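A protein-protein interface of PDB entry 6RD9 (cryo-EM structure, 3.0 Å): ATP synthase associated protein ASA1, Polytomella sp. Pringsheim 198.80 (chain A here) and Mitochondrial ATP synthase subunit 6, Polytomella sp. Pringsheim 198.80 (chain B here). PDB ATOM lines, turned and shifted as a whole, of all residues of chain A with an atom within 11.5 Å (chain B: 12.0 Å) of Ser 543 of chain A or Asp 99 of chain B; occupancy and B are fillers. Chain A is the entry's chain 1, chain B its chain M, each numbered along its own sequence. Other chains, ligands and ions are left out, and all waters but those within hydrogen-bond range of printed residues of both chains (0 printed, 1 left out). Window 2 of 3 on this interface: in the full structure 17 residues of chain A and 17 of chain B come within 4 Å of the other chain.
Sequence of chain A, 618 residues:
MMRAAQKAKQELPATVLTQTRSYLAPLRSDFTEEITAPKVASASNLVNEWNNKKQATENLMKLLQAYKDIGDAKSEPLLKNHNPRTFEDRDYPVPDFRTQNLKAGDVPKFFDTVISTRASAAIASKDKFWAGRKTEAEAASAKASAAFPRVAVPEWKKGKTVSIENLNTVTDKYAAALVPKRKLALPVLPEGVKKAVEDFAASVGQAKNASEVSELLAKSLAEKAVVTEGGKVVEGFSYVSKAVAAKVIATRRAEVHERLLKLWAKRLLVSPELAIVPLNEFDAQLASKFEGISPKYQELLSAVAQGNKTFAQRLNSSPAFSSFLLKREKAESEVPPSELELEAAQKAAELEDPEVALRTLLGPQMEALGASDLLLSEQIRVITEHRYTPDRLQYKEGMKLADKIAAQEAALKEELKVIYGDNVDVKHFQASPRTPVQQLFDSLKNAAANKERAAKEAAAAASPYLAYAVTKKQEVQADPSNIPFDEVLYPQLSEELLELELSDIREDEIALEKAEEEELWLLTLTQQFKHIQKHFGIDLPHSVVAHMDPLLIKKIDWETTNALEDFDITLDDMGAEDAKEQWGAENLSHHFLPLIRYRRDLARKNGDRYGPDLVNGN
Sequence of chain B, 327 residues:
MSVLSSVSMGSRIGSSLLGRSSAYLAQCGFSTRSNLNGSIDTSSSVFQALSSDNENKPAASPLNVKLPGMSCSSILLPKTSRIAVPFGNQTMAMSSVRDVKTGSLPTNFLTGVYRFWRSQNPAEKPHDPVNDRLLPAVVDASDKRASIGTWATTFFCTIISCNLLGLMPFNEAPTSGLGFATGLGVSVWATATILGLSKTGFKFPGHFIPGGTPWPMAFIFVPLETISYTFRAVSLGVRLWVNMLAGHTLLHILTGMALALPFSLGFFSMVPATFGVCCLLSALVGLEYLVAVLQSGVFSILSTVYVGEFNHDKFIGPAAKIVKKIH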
ATOM      1  N   PRO A 319      15.263 -21.729  16.959  1.00  0.00           N
ATOM      2  CA  PRO A 319      15.145 -20.381  17.519  1.00  0.00           C
ATOM      3  C   PRO A 319      15.677 -20.249  18.925  1.00  0.00           C
ATOM      4  O   PRO A 319      15.867 -19.127  19.388  1.00  0.00           O
ATOM      5  CB  PRO A 319      13.643 -20.125  17.470  1.00  0.00           C
ATOM      6  CG  PRO A 319      13.169 -20.950  16.406  1.00  0.00           C
ATOM      7  CD  PRO A 319      13.984 -22.173  16.394  1.00  0.00           C
ATOM      8  N   GLN A 528       3.898 -37.341   6.636  1.00  0.00           N
ATOM      9  CA  GLN A 528       3.456 -36.517   7.745  1.00  0.00           C
ATOM     10  C   GLN A 528       4.189 -36.864   9.029  1.00  0.00           C
ATOM     11  O   GLN A 528       4.573 -35.965   9.770  1.00  0.00           O
ATOM     12  CB  GLN A 528       1.958 -36.659   7.902  1.00  0.00           C
ATOM     13  CG  GLN A 528       1.447 -36.374   9.235  1.00  0.00           C
ATOM     14  CD  GLN A 528       0.017 -36.673   9.334  1.00  0.00           C
ATOM     15  OE1 GLN A 528      -0.715 -36.517   8.380  1.00  0.00           O
ATOM     16  NE2 GLN A 528      -0.407 -37.112  10.496  1.00  0.00           N
ATOM     17  N   HIS A 531       7.786 -35.517   8.967  1.00  0.00           N
ATOM     18  CA  HIS A 531       7.928 -34.092   9.162  1.00  0.00           C
ATOM     19  C   HIS A 531       7.688 -33.687  10.594  1.00  0.00           C
ATOM     20  O   HIS A 531       8.301 -32.734  11.062  1.00  0.00           O
ATOM     21  CB  HIS A 531       6.976 -33.344   8.261  1.00  0.00           C
ATOM     22  CG  HIS A 531       7.206 -31.877   8.249  1.00  0.00           C
ATOM     23  ND1 HIS A 531       6.303 -30.985   8.763  1.00  0.00           N
ATOM     24  CD2 HIS A 531       8.253 -31.147   7.821  1.00  0.00           C
ATOM     25  CE1 HIS A 531       6.771 -29.763   8.627  1.00  0.00           C
ATOM     26  NE2 HIS A 531       7.954 -29.833   8.054  1.00  0.00           N
ATOM     27  N   ILE A 532       6.805 -34.379  11.302  1.00  0.00           N
ATOM     28  CA  ILE A 532       6.672 -34.151  12.729  1.00  0.00           C
ATOM     29  C   ILE A 532       7.944 -34.560  13.439  1.00  0.00           C
ATOM     30  O   ILE A 532       8.521 -33.767  14.171  1.00  0.00           O
ATOM     31  CB  ILE A 532       5.455 -34.893  13.286  1.00  0.00           C
ATOM     32  CG1 ILE A 532       4.197 -34.353  12.659  1.00  0.00           C
ATOM     33  CG2 ILE A 532       5.339 -34.653  14.707  1.00  0.00           C
ATOM     34  CD1 ILE A 532       2.976 -35.100  13.026  1.00  0.00           C
ATOM     35  N   HIS A 535      10.962 -32.284  13.236  1.00  0.00           N
ATOM     36  CA  HIS A 535      10.783 -30.938  13.731  1.00  0.00           C
ATOM     37  C   HIS A 535      10.138 -30.840  15.098  1.00  0.00           C
ATOM     38  O   HIS A 535      10.103 -29.743  15.638  1.00  0.00           O
ATOM     39  CB  HIS A 535       9.925 -30.130  12.753  1.00  0.00           C
ATOM     40  CG  HIS A 535      10.639 -29.723  11.509  1.00  0.00           C
ATOM     41  ND1 HIS A 535      11.636 -28.779  11.505  1.00  0.00           N
ATOM     42  CD2 HIS A 535      10.485 -30.109  10.228  1.00  0.00           C
ATOM     43  CE1 HIS A 535      12.082 -28.620  10.278  1.00  0.00           C
ATOM     44  NE2 HIS A 535      11.398 -29.414   9.483  1.00  0.00           N
ATOM     45  N   PHE A 536       9.603 -31.917  15.657  1.00  0.00           N
ATOM     46  CA  PHE A 536       8.911 -31.828  16.934  1.00  0.00           C
ATOM     47  C   PHE A 536       9.900 -31.604  18.049  1.00  0.00           C
ATOM     48  O   PHE A 536      10.900 -32.314  18.149  1.00  0.00           O
ATOM     49  CB  PHE A 536       8.133 -33.099  17.214  1.00  0.00           C
ATOM     50  CG  PHE A 536       7.220 -32.999  18.362  1.00  0.00           C
ATOM     51  CD1 PHE A 536       6.045 -32.320  18.255  1.00  0.00           C
ATOM     52  CD2 PHE A 536       7.533 -33.591  19.550  1.00  0.00           C
ATOM     53  CE1 PHE A 536       5.223 -32.225  19.304  1.00  0.00           C
ATOM     54  CE2 PHE A 536       6.712 -33.490  20.584  1.00  0.00           C
ATOM     55  CZ  PHE A 536       5.556 -32.811  20.466  1.00  0.00           C
ATOM     56  N   ILE A 538      11.778 -29.081  18.345  1.00  0.00           N
ATOM     57  CA  ILE A 538      12.857 -28.229  17.887  1.00  0.00           C
ATOM     58  C   ILE A 538      12.250 -26.947  17.359  1.00  0.00           C
ATOM     59  O   ILE A 538      12.410 -25.892  17.967  1.00  0.00           O
ATOM     60  CB  ILE A 538      13.713 -28.926  16.822  1.00  0.00           C
ATOM     61  CG1 ILE A 538      14.447 -30.104  17.419  1.00  0.00           C
ATOM     62  CG2 ILE A 538      14.722 -28.006  16.290  1.00  0.00           C
ATOM     63  CD1 ILE A 538      14.846 -31.093  16.429  1.00  0.00           C
ATOM     64  N   ASP A 539      11.526 -27.011  16.254  1.00  0.00           N
ATOM     65  CA  ASP A 539      10.958 -25.781  15.731  1.00  0.00           C
ATOM     66  C   ASP A 539       9.583 -25.924  15.110  1.00  0.00           C
ATOM     67  O   ASP A 539       9.179 -25.021  14.387  1.00  0.00           O
ATOM     68  CB  ASP A 539      11.884 -25.121  14.705  1.00  0.00           C
ATOM     69  CG  ASP A 539      12.470 -26.097  13.699  1.00  0.00           C
ATOM     70  OD1 ASP A 539      11.813 -27.072  13.329  1.00  0.00           O
ATOM     71  OD2 ASP A 539      13.608 -25.880  13.255  1.00  0.00           O
ATOM     72  N   LEU A 540       8.867 -27.001  15.328  1.00  0.00           N
ATOM     73  CA  LEU A 540       7.599 -27.177  14.639  1.00  0.00           C
ATOM     74  C   LEU A 540       6.563 -26.274  15.272  1.00  0.00           C
ATOM     75  O   LEU A 540       6.434 -26.274  16.486  1.00  0.00           O
ATOM     76  CB  LEU A 540       7.147 -28.618  14.734  1.00  0.00           C
ATOM     77  CG  LEU A 540       5.967 -29.233  13.996  1.00  0.00           C
ATOM     78  CD1 LEU A 540       6.124 -29.144  12.555  1.00  0.00           C
ATOM     79  CD2 LEU A 540       5.920 -30.626  14.383  1.00  0.00           C
ATOM     80  N   PRO A 541       5.842 -25.472  14.511  1.00  0.00           N
ATOM     81  CA  PRO A 541       4.778 -24.697  15.115  1.00  0.00           C
ATOM     82  C   PRO A 541       3.587 -25.565  15.440  1.00  0.00           C
ATOM     83  O   PRO A 541       3.406 -26.651  14.912  1.00  0.00           O
ATOM     84  CB  PRO A 541       4.446 -23.662  14.047  1.00  0.00           C
ATOM     85  CG  PRO A 541       5.022 -24.098  12.891  1.00  0.00           C
ATOM     86  CD  PRO A 541       6.155 -24.953  13.185  1.00  0.00           C
ATOM     87  N   HIS A 542       2.776 -25.078  16.353  1.00  0.00           N
ATOM     88  CA  HIS A 542       1.543 -25.755  16.675  1.00  0.00           C
ATOM     89  C   HIS A 542       0.502 -25.626  15.594  1.00  0.00           C
ATOM     90  O   HIS A 542      -0.483 -26.358  15.622  1.00  0.00           O
ATOM     91  CB  HIS A 542       0.984 -25.195  17.958  1.00  0.00           C
ATOM     92  CG  HIS A 542       1.473 -25.879  19.182  1.00  0.00           C
ATOM     93  ND1 HIS A 542       2.743 -25.709  19.662  1.00  0.00           N
ATOM     94  CD2 HIS A 542       0.840 -26.664  20.071  1.00  0.00           C
ATOM     95  CE1 HIS A 542       2.888 -26.398  20.771  1.00  0.00           C
ATOM     96  NE2 HIS A 542       1.745 -26.984  21.044  1.00  0.00           N
ATOM     97  N   SER A 543       0.673 -24.695  14.668  1.00  0.00           N
ATOM     98  CA  SER A 543      -0.283 -24.549  13.586  1.00  0.00           C
ATOM     99  C   SER A 543      -0.091 -25.613  12.542  1.00  0.00           C
ATOM    100  O   SER A 543      -1.036 -25.967  11.844  1.00  0.00           O
ATOM    101  CB  SER A 543      -0.126 -23.195  12.947  1.00  0.00           C
ATOM    102  OG  SER A 543       1.234 -22.880  12.843  1.00  0.00           O
ATOM    103  N   VAL A 544       1.133 -26.104  12.403  1.00  0.00           N
ATOM    104  CA  VAL A 544       1.458 -27.100  11.404  1.00  0.00           C
ATOM    105  C   VAL A 544       1.065 -28.471  11.888  1.00  0.00           C
ATOM    106  O   VAL A 544       0.625 -29.303  11.100  1.00  0.00           O
ATOM    107  CB  VAL A 544       2.946 -26.981  11.057  1.00  0.00           C
ATOM    108  CG1 VAL A 544       3.413 -28.087  10.226  1.00  0.00           C
ATOM    109  CG2 VAL A 544       3.132 -25.765  10.277  1.00  0.00           C
ATOM    110  N   VAL A 545       1.157 -28.713  13.187  1.00  0.00           N
ATOM    111  CA  VAL A 545       0.657 -29.949  13.773  1.00  0.00           C
ATOM    112  C   VAL A 545      -0.846 -30.042  13.607  1.00  0.00           C
ATOM    113  O   VAL A 545      -1.381 -31.067  13.190  1.00  0.00           O
ATOM    114  CB  VAL A 545       1.042 -30.015  15.251  1.00  0.00           C
ATOM    115  CG1 VAL A 545       0.389 -31.151  15.881  1.00  0.00           C
ATOM    116  CG2 VAL A 545       2.475 -30.128  15.396  1.00  0.00           C
ATOM    117  N   ALA A 546      -1.552 -28.968  13.911  1.00  0.00           N
ATOM    118  CA  ALA A 546      -2.995 -28.973  13.787  1.00  0.00           C
ATOM    119  C   ALA A 546      -3.445 -28.905  12.353  1.00  0.00           C
ATOM    120  O   ALA A 546      -4.622 -29.124  12.079  1.00  0.00           O
ATOM    121  CB  ALA A 546      -3.582 -27.808  14.555  1.00  0.00           C
ATOM    122  N   HIS A 547      -2.557 -28.553  11.438  1.00  0.00           N
ATOM    123  CA  HIS A 547      -2.875 -28.660  10.031  1.00  0.00           C
ATOM    124  C   HIS A 547      -2.719 -30.086   9.568  1.00  0.00           C
ATOM    125  O   HIS A 547      -3.635 -30.657   8.985  1.00  0.00           O
ATOM    126  CB  HIS A 547      -1.973 -27.754   9.216  1.00  0.00           C
ATOM    127  CG  HIS A 547      -2.266 -27.798   7.759  1.00  0.00           C
ATOM    128  ND1 HIS A 547      -1.454 -28.432   6.854  1.00  0.00           N
ATOM    129  CD2 HIS A 547      -3.308 -27.312   7.054  1.00  0.00           C
ATOM    130  CE1 HIS A 547      -1.975 -28.327   5.650  1.00  0.00           C
ATOM    131  NE2 HIS A 547      -3.104 -27.654   5.744  1.00  0.00           N
ATOM    132  N   MET A 548      -1.565 -30.674   9.853  1.00  0.00           N
ATOM    133  CA  MET A 548      -1.259 -32.023   9.428  1.00  0.00           C
ATOM    134  C   MET A 548      -2.159 -33.035  10.098  1.00  0.00           C
ATOM    135  O   MET A 548      -2.687 -33.931   9.445  1.00  0.00           O
ATOM    136  CB  MET A 548       0.185 -32.338   9.747  1.00  0.00           C
ATOM    137  CG  MET A 548       1.143 -31.918   8.750  1.00  0.00           C
ATOM    138  SD  MET A 548       2.608 -32.833   9.075  1.00  0.00           S
ATOM    139  CE  MET A 548       3.321 -31.780  10.266  1.00  0.00           C
ATOM    140  N   ASP A 549      -2.358 -32.916  11.398  1.00  0.00           N
ATOM    141  CA  ASP A 549      -3.156 -33.873  12.147  1.00  0.00           C
ATOM    142  C   ASP A 549      -4.271 -33.128  12.851  1.00  0.00           C
ATOM    143  O   ASP A 549      -4.139 -32.770  14.021  1.00  0.00           O
ATOM    144  CB  ASP A 549      -2.300 -34.638  13.140  1.00  0.00           C
ATOM    145  CG  ASP A 549      -2.716 -36.065  13.248  1.00  0.00           C
ATOM    146  OD1 ASP A 549      -3.747 -36.404  12.661  1.00  0.00           O
ATOM    147  OD2 ASP A 549      -1.988 -36.867  13.856  1.00  0.00           O
ATOM    148  N   PRO A 550      -5.378 -32.861  12.165  1.00  0.00           N
ATOM    149  CA  PRO A 550      -6.425 -32.066  12.789  1.00  0.00           C
ATOM    150  C   PRO A 550      -7.279 -32.843  13.753  1.00  0.00           C
ATOM    151  O   PRO A 550      -7.822 -32.246  14.680  1.00  0.00           O
ATOM    152  CB  PRO A 550      -7.230 -31.579  11.589  1.00  0.00           C
ATOM    153  CG  PRO A 550      -7.028 -32.554  10.600  1.00  0.00           C
ATOM    154  CD  PRO A 550      -5.673 -33.098  10.751  1.00  0.00           C
ATOM    155  N   LEU A 551      -7.437 -34.139  13.564  1.00  0.00           N
ATOM    156  CA  LEU A 551      -8.248 -34.930  14.463  1.00  0.00           C
ATOM    157  C   LEU A 551      -7.473 -35.444  15.645  1.00  0.00           C
ATOM    158  O   LEU A 551      -8.079 -35.983  16.556  1.00  0.00           O
ATOM    159  CB  LEU A 551      -8.853 -36.123  13.738  1.00  0.00           C
ATOM    160  CG  LEU A 551      -9.835 -35.924  12.608  1.00  0.00           C
ATOM    161  CD1 LEU A 551     -10.281 -37.247  12.141  1.00  0.00           C
ATOM    162  CD2 LEU A 551     -10.991 -35.173  13.105  1.00  0.00           C
ATOM    163  N   LEU A 552      -6.157 -35.354  15.636  1.00  0.00           N
ATOM    164  CA  LEU A 552      -5.415 -35.643  16.851  1.00  0.00           C
ATOM    165  C   LEU A 552      -5.499 -34.478  17.799  1.00  0.00           C
ATOM    166  O   LEU A 552      -5.684 -34.657  18.997  1.00  0.00           O
ATOM    167  CB  LEU A 552      -3.962 -35.942  16.537  1.00  0.00           C
ATOM    168  CG  LEU A 552      -3.088 -36.229  17.737  1.00  0.00           C
ATOM    169  CD1 LEU A 552      -3.529 -37.466  18.406  1.00  0.00           C
ATOM    170  CD2 LEU A 552      -1.690 -36.349  17.340  1.00  0.00           C
ATOM    171  N   ILE A 553      -5.385 -33.271  17.264  1.00  0.00           N
ATOM    172  CA  ILE A 553      -5.569 -32.052  18.027  1.00  0.00           C
ATOM    173  C   ILE A 553      -6.997 -31.930  18.514  1.00  0.00           C
ATOM    174  O   ILE A 553      -7.231 -31.467  19.622  1.00  0.00           O
ATOM    175  CB  ILE A 553      -5.133 -30.883  17.137  1.00  0.00           C
ATOM    176  CG1 ILE A 553      -3.645 -30.978  16.862  1.00  0.00           C
ATOM    177  CG2 ILE A 553      -5.481 -29.579  17.699  1.00  0.00           C
ATOM    178  CD1 ILE A 553      -2.809 -31.071  18.061  1.00  0.00           C
ATOM    179  N   LYS A 554      -7.964 -32.394  17.735  1.00  0.00           N
ATOM    180  CA  LYS A 554      -9.363 -32.365  18.136  1.00  0.00           C
ATOM    181  C   LYS A 554      -9.631 -33.280  19.313  1.00  0.00           C
ATOM    182  O   LYS A 554     -10.406 -32.936  20.201  1.00  0.00           O
ATOM    183  CB  LYS A 554     -10.237 -32.770  16.964  1.00  0.00           C
ATOM    184  CG  LYS A 554     -11.698 -32.682  17.214  1.00  0.00           C
ATOM    185  CD  LYS A 554     -12.429 -33.630  16.350  1.00  0.00           C
ATOM    186  CE  LYS A 554     -13.877 -33.561  16.598  1.00  0.00           C
ATOM    187  NZ  LYS A 554     -14.546 -34.656  15.885  1.00  0.00           N
ATOM    188  N   ASP A 557      -7.801 -31.852  22.480  1.00  0.00           N
ATOM    189  CA  ASP A 557      -8.610 -30.772  23.016  1.00  0.00           C
ATOM    190  C   ASP A 557      -9.858 -31.256  23.705  1.00  0.00           C
ATOM    191  O   ASP A 557     -10.447 -30.501  24.465  1.00  0.00           O
ATOM    192  CB  ASP A 557      -9.041 -29.832  21.913  1.00  0.00           C
ATOM    193  CG  ASP A 557      -7.926 -29.025  21.381  1.00  0.00           C
ATOM    194  OD1 ASP A 557      -6.795 -29.219  21.836  1.00  0.00           O
ATOM    195  OD2 ASP A 557      -8.178 -28.185  20.509  1.00  0.00           O
ATOM    196  N   SER B  95      -9.365 -13.422  18.426  1.00  0.00           N
ATOM    197  CA  SER B  95     -10.150 -14.340  17.608  1.00  0.00           C
ATOM    198  C   SER B  95      -9.225 -15.274  16.832  1.00  0.00           C
ATOM    199  O   SER B  95      -9.596 -16.391  16.475  1.00  0.00           O
ATOM    200  CB  SER B  95     -11.062 -13.560  16.662  1.00  0.00           C
ATOM    201  OG  SER B  95     -11.874 -12.652  17.387  1.00  0.00           O
ATOM    202  N   SER B  96      -8.016 -14.789  16.577  1.00  0.00           N
ATOM    203  CA  SER B  96      -6.927 -15.572  16.014  1.00  0.00           C
ATOM    204  C   SER B  96      -5.901 -15.765  17.119  1.00  0.00           C
ATOM    205  O   SER B  96      -5.340 -14.791  17.627  1.00  0.00           O
ATOM    206  CB  SER B  96      -6.314 -14.866  14.809  1.00  0.00           C
ATOM    207  OG  SER B  96      -5.112 -15.493  14.402  1.00  0.00           O
ATOM    208  N   VAL B  97      -5.664 -17.007  17.501  1.00  0.00           N
ATOM    209  CA  VAL B  97      -4.733 -17.265  18.580  1.00  0.00           C
ATOM    210  C   VAL B  97      -3.309 -17.240  18.052  1.00  0.00           C
ATOM    211  O   VAL B  97      -3.058 -17.312  16.854  1.00  0.00           O
ATOM    212  CB  VAL B  97      -5.046 -18.592  19.268  1.00  0.00           C
ATOM    213  CG1 VAL B  97      -6.465 -18.587  19.677  1.00  0.00           C
ATOM    214  CG2 VAL B  97      -4.777 -19.703  18.344  1.00  0.00           C
ATOM    215  N   ARG B  98      -2.366 -17.109  18.967  1.00  0.00           N
ATOM    216  CA  ARG B  98      -0.989 -17.031  18.553  1.00  0.00           C
ATOM    217  C   ARG B  98      -0.449 -18.418  18.288  1.00  0.00           C
ATOM    218  O   ARG B  98      -1.043 -19.422  18.661  1.00  0.00           O
ATOM    219  CB  ARG B  98      -0.147 -16.326  19.604  1.00  0.00           C
ATOM    220  CG  ARG B  98       0.118 -17.126  20.837  1.00  0.00           C
ATOM    221  CD  ARG B  98       0.490 -16.212  21.963  1.00  0.00           C
ATOM    222  NE  ARG B  98      -0.454 -15.111  22.069  1.00  0.00           N
ATOM    223  CZ  ARG B  98      -0.297 -14.078  22.876  1.00  0.00           C
ATOM    224  NH1 ARG B  98       0.763 -14.004  23.651  1.00  0.00           N
ATOM    225  NH2 ARG B  98      -1.202 -13.121  22.904  1.00  0.00           N
ATOM    226  N   ASP B  99       0.684 -18.462  17.617  1.00  0.00           N
ATOM    227  CA  ASP B  99       1.325 -19.711  17.260  1.00  0.00           C
ATOM    228  C   ASP B  99       2.442 -19.992  18.235  1.00  0.00           C
ATOM    229  O   ASP B  99       3.190 -19.095  18.618  1.00  0.00           O
ATOM    230  CB  ASP B  99       1.882 -19.657  15.848  1.00  0.00           C
ATOM    231  CG  ASP B  99       1.994 -21.001  15.232  1.00  0.00           C
ATOM    232  OD1 ASP B  99       1.938 -21.988  15.960  1.00  0.00           O
ATOM    233  OD2 ASP B  99       2.148 -21.082  14.013  1.00  0.00           O
ATOM    234  N   VAL B 100       2.553 -21.244  18.629  1.00  0.00           N
ATOM    235  CA  VAL B 100       3.492 -21.661  19.644  1.00  0.00           C
ATOM    236  C   VAL B 100       4.482 -22.589  18.983  1.00  0.00           C
ATOM    237  O   VAL B 100       4.090 -23.471  18.224  1.00  0.00           O
ATOM    238  CB  VAL B 100       2.782 -22.370  20.802  1.00  0.00           C
ATOM    239  CG1 VAL B 100       3.736 -22.596  21.912  1.00  0.00           C
ATOM    240  CG2 VAL B 100       1.626 -21.576  21.256  1.00  0.00           C
ATOM    241  N   LYS B 101       5.753 -22.379  19.239  1.00  0.00           N
ATOM    242  CA  LYS B 101       6.742 -23.359  18.851  1.00  0.00           C
ATOM    243  C   LYS B 101       6.666 -24.536  19.792  1.00  0.00           C
ATOM    244  O   LYS B 101       6.499 -24.360  20.996  1.00  0.00           O
ATOM    245  CB  LYS B 101       8.114 -22.734  18.911  1.00  0.00           C
ATOM    246  CG  LYS B 101       9.222 -23.626  18.546  1.00  0.00           C
ATOM    247  CD  LYS B 101      10.415 -22.809  18.296  1.00  0.00           C
ATOM    248  CE  LYS B 101      10.950 -22.282  19.549  1.00  0.00           C
ATOM    249  NZ  LYS B 101      11.754 -23.330  20.153  1.00  0.00           N
ATOM    250  N   THR B 102       6.759 -25.746  19.256  1.00  0.00           N
ATOM    251  CA  THR B 102       6.779 -26.900  20.134  1.00  0.00           C
ATOM    252  C   THR B 102       8.132 -26.975  20.798  1.00  0.00           C
ATOM    253  O   THR B 102       9.141 -26.612  20.207  1.00  0.00           O
ATOM    254  CB  THR B 102       6.517 -28.201  19.395  1.00  0.00           C
ATOM    255  OG1 THR B 102       7.508 -28.381  18.401  1.00  0.00           O
ATOM    256  CG2 THR B 102       5.179 -28.201  18.756  1.00  0.00           C
ATOM    257  N   GLY B 103       8.147 -27.418  22.045  1.00  0.00           N
ATOM    258  CA  GLY B 103       9.399 -27.584  22.735  1.00  0.00           C
ATOM    259  C   GLY B 103      10.043 -26.298  23.156  1.00  0.00           C
ATOM    260  O   GLY B 103      11.264 -26.241  23.272  1.00  0.00           O
ATOM    261  N   SER B 104       9.252 -25.255  23.373  1.00  0.00           N
ATOM    262  CA  SER B 104       9.742 -24.017  23.936  1.00  0.00           C
ATOM    263  C   SER B 104      10.168 -24.247  25.365  1.00  0.00           C
ATOM    264  O   SER B 104       9.700 -25.166  26.017  1.00  0.00           O
ATOM    265  CB  SER B 104       8.651 -22.974  23.916  1.00  0.00           C
ATOM    266  OG  SER B 104       8.342 -22.609  22.605  1.00  0.00           O
ATOM    267  N   LEU B 105      11.054 -23.406  25.865  1.00  0.00           N
ATOM    268  CA  LEU B 105      11.436 -23.514  27.269  1.00  0.00           C
ATOM    269  C   LEU B 105      10.329 -23.174  28.267  1.00  0.00           C
ATOM    270  O   LEU B 105      10.294 -23.827  29.322  1.00  0.00           O
ATOM    271  CB  LEU B 105      12.696 -22.681  27.513  1.00  0.00           C
ATOM    272  CG  LEU B 105      13.346 -22.626  28.880  1.00  0.00           C
ATOM    273  CD1 LEU B 105      14.801 -22.606  28.729  1.00  0.00           C
ATOM    274  CD2 LEU B 105      12.959 -21.361  29.565  1.00  0.00           C
ATOM    275  N   PRO B 106       9.437 -22.194  28.058  1.00  0.00           N
ATOM    276  CA  PRO B 106       8.325 -22.064  29.003  1.00  0.00           C
ATOM    277  C   PRO B 106       7.305 -23.173  28.919  1.00  0.00           C
ATOM    278  O   PRO B 106       6.593 -23.412  29.891  1.00  0.00           O
ATOM    279  CB  PRO B 106       7.715 -20.721  28.621  1.00  0.00           C
ATOM    280  CG  PRO B 106       8.777 -20.015  28.054  1.00  0.00           C
ATOM    281  CD  PRO B 106       9.511 -20.966  27.253  1.00  0.00           C
ATOM    282  N   THR B 107       7.197 -23.843  27.783  1.00  0.00           N
ATOM    283  CA  THR B 107       6.317 -24.993  27.653  1.00  0.00           C
ATOM    284  C   THR B 107       6.909 -26.199  28.348  1.00  0.00           C
ATOM    285  O   THR B 107       6.185 -27.019  28.902  1.00  0.00           O
ATOM    286  CB  THR B 107       6.094 -25.266  26.173  1.00  0.00           C
ATOM    287  OG1 THR B 107       5.650 -24.066  25.546  1.00  0.00           O
ATOM    288  CG2 THR B 107       5.075 -26.318  25.936  1.00  0.00           C
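Printed residues of chain B within 4 Å of Ile 538 of chain A: Lys 101. Ser 543 of chain A touches one residue of chain B. No residue of chain B comes within 4 Å of Val 544 of chain A. No residue of chain A comes within 4 Å of Val 97 of chain B. Of chain A, only Pro 541, His 542 and Ser 543 come within 4 Å of Asp 99 of chain B. Val 100 of chain B touches two residues of chain A. Of the printed residues of chain A, Thr 102 of chain B touches Leu 540 and His 542. Pro 106 of chain B touches none of the printed residues of chain A. The nearest residue of chain B that does not touch Ser 543 of chain A is Val 100 of chain B (5.1 Å). The nearest residue of chain A that does not touch Asp 99 of chain B is Val 544 of chain A (5.4 Å).
OG of Ser 104 of chain B lies within hydrogen-bond range of O of Lys 101 of chain B (3.0 Å). The side-chain carboxylate of Asp 539 of chain A sits at hydrogen-bond distance from a ring nitrogen (ND1) of His 535 of chain A (2.5 Å). O of His 535 of chain A sits at hydrogen-bond distance from N of Leu 540 of chain A, at 3.0 Å.
Of the 24 printed residues of chain A, 7 touch a printed residue of chain B. Hydrophobic or aromatic side chains of chain A within 4 Å of the printed part of chain B: Pro 319, Leu 540, Pro 541 and His 542. Of the 13 printed residues of chain B, 4 touch a printed residue of chain A. Printed residues of chain B that touch a printed residue of chain A: Asp 99, Val 100, Lys 101 and Thr 102. Hydrophobic or aromatic side chains of chain B within 4 Å of the printed part of chain A: Val 100. Among the printed residues, 11 pairs touch across the chains. Among the printed residues, no Asp or Glu carboxylate lies within 4 Å of a Lys or Arg side-chain nitrogen of the other chain.
Among the printed residues, merely in contact across the chains: Pro 319 of chain A with Lys 101 of chain B, Asp 539 of chain A with Lys 101 of chain B, Leu 540 of chain A with Lys 101 of chain B, Pro 541 of chain A with Asp 99 of chain B, Pro 541 of chain A with Val 100 of chain B and His 542 of chain A with Thr 102 of chain B.
N of His 542 of chain A is in hydrogen-bond range of OD1 of Asp 99 of chain B, at 3.2 Å. N of Ser 543 of chain A lies within hydrogen-bond range of OD1 of Asp 99 of chain B, at 3.3 Å. N of His 542 of chain A sits at hydrogen-bond distance from O of Val 100 of chain B, at 2.8 Å. The side-chain amino group (NZ) of Lys 101 of chain B lies within hydrogen-bond range of the backbone carbonyl oxygen (O) of Ile 538 of chain A, 3.4 Å away. N of Thr 102 of chain B lies within hydrogen-bond range of O of Leu 540 of chain A, 2.8 Å away.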
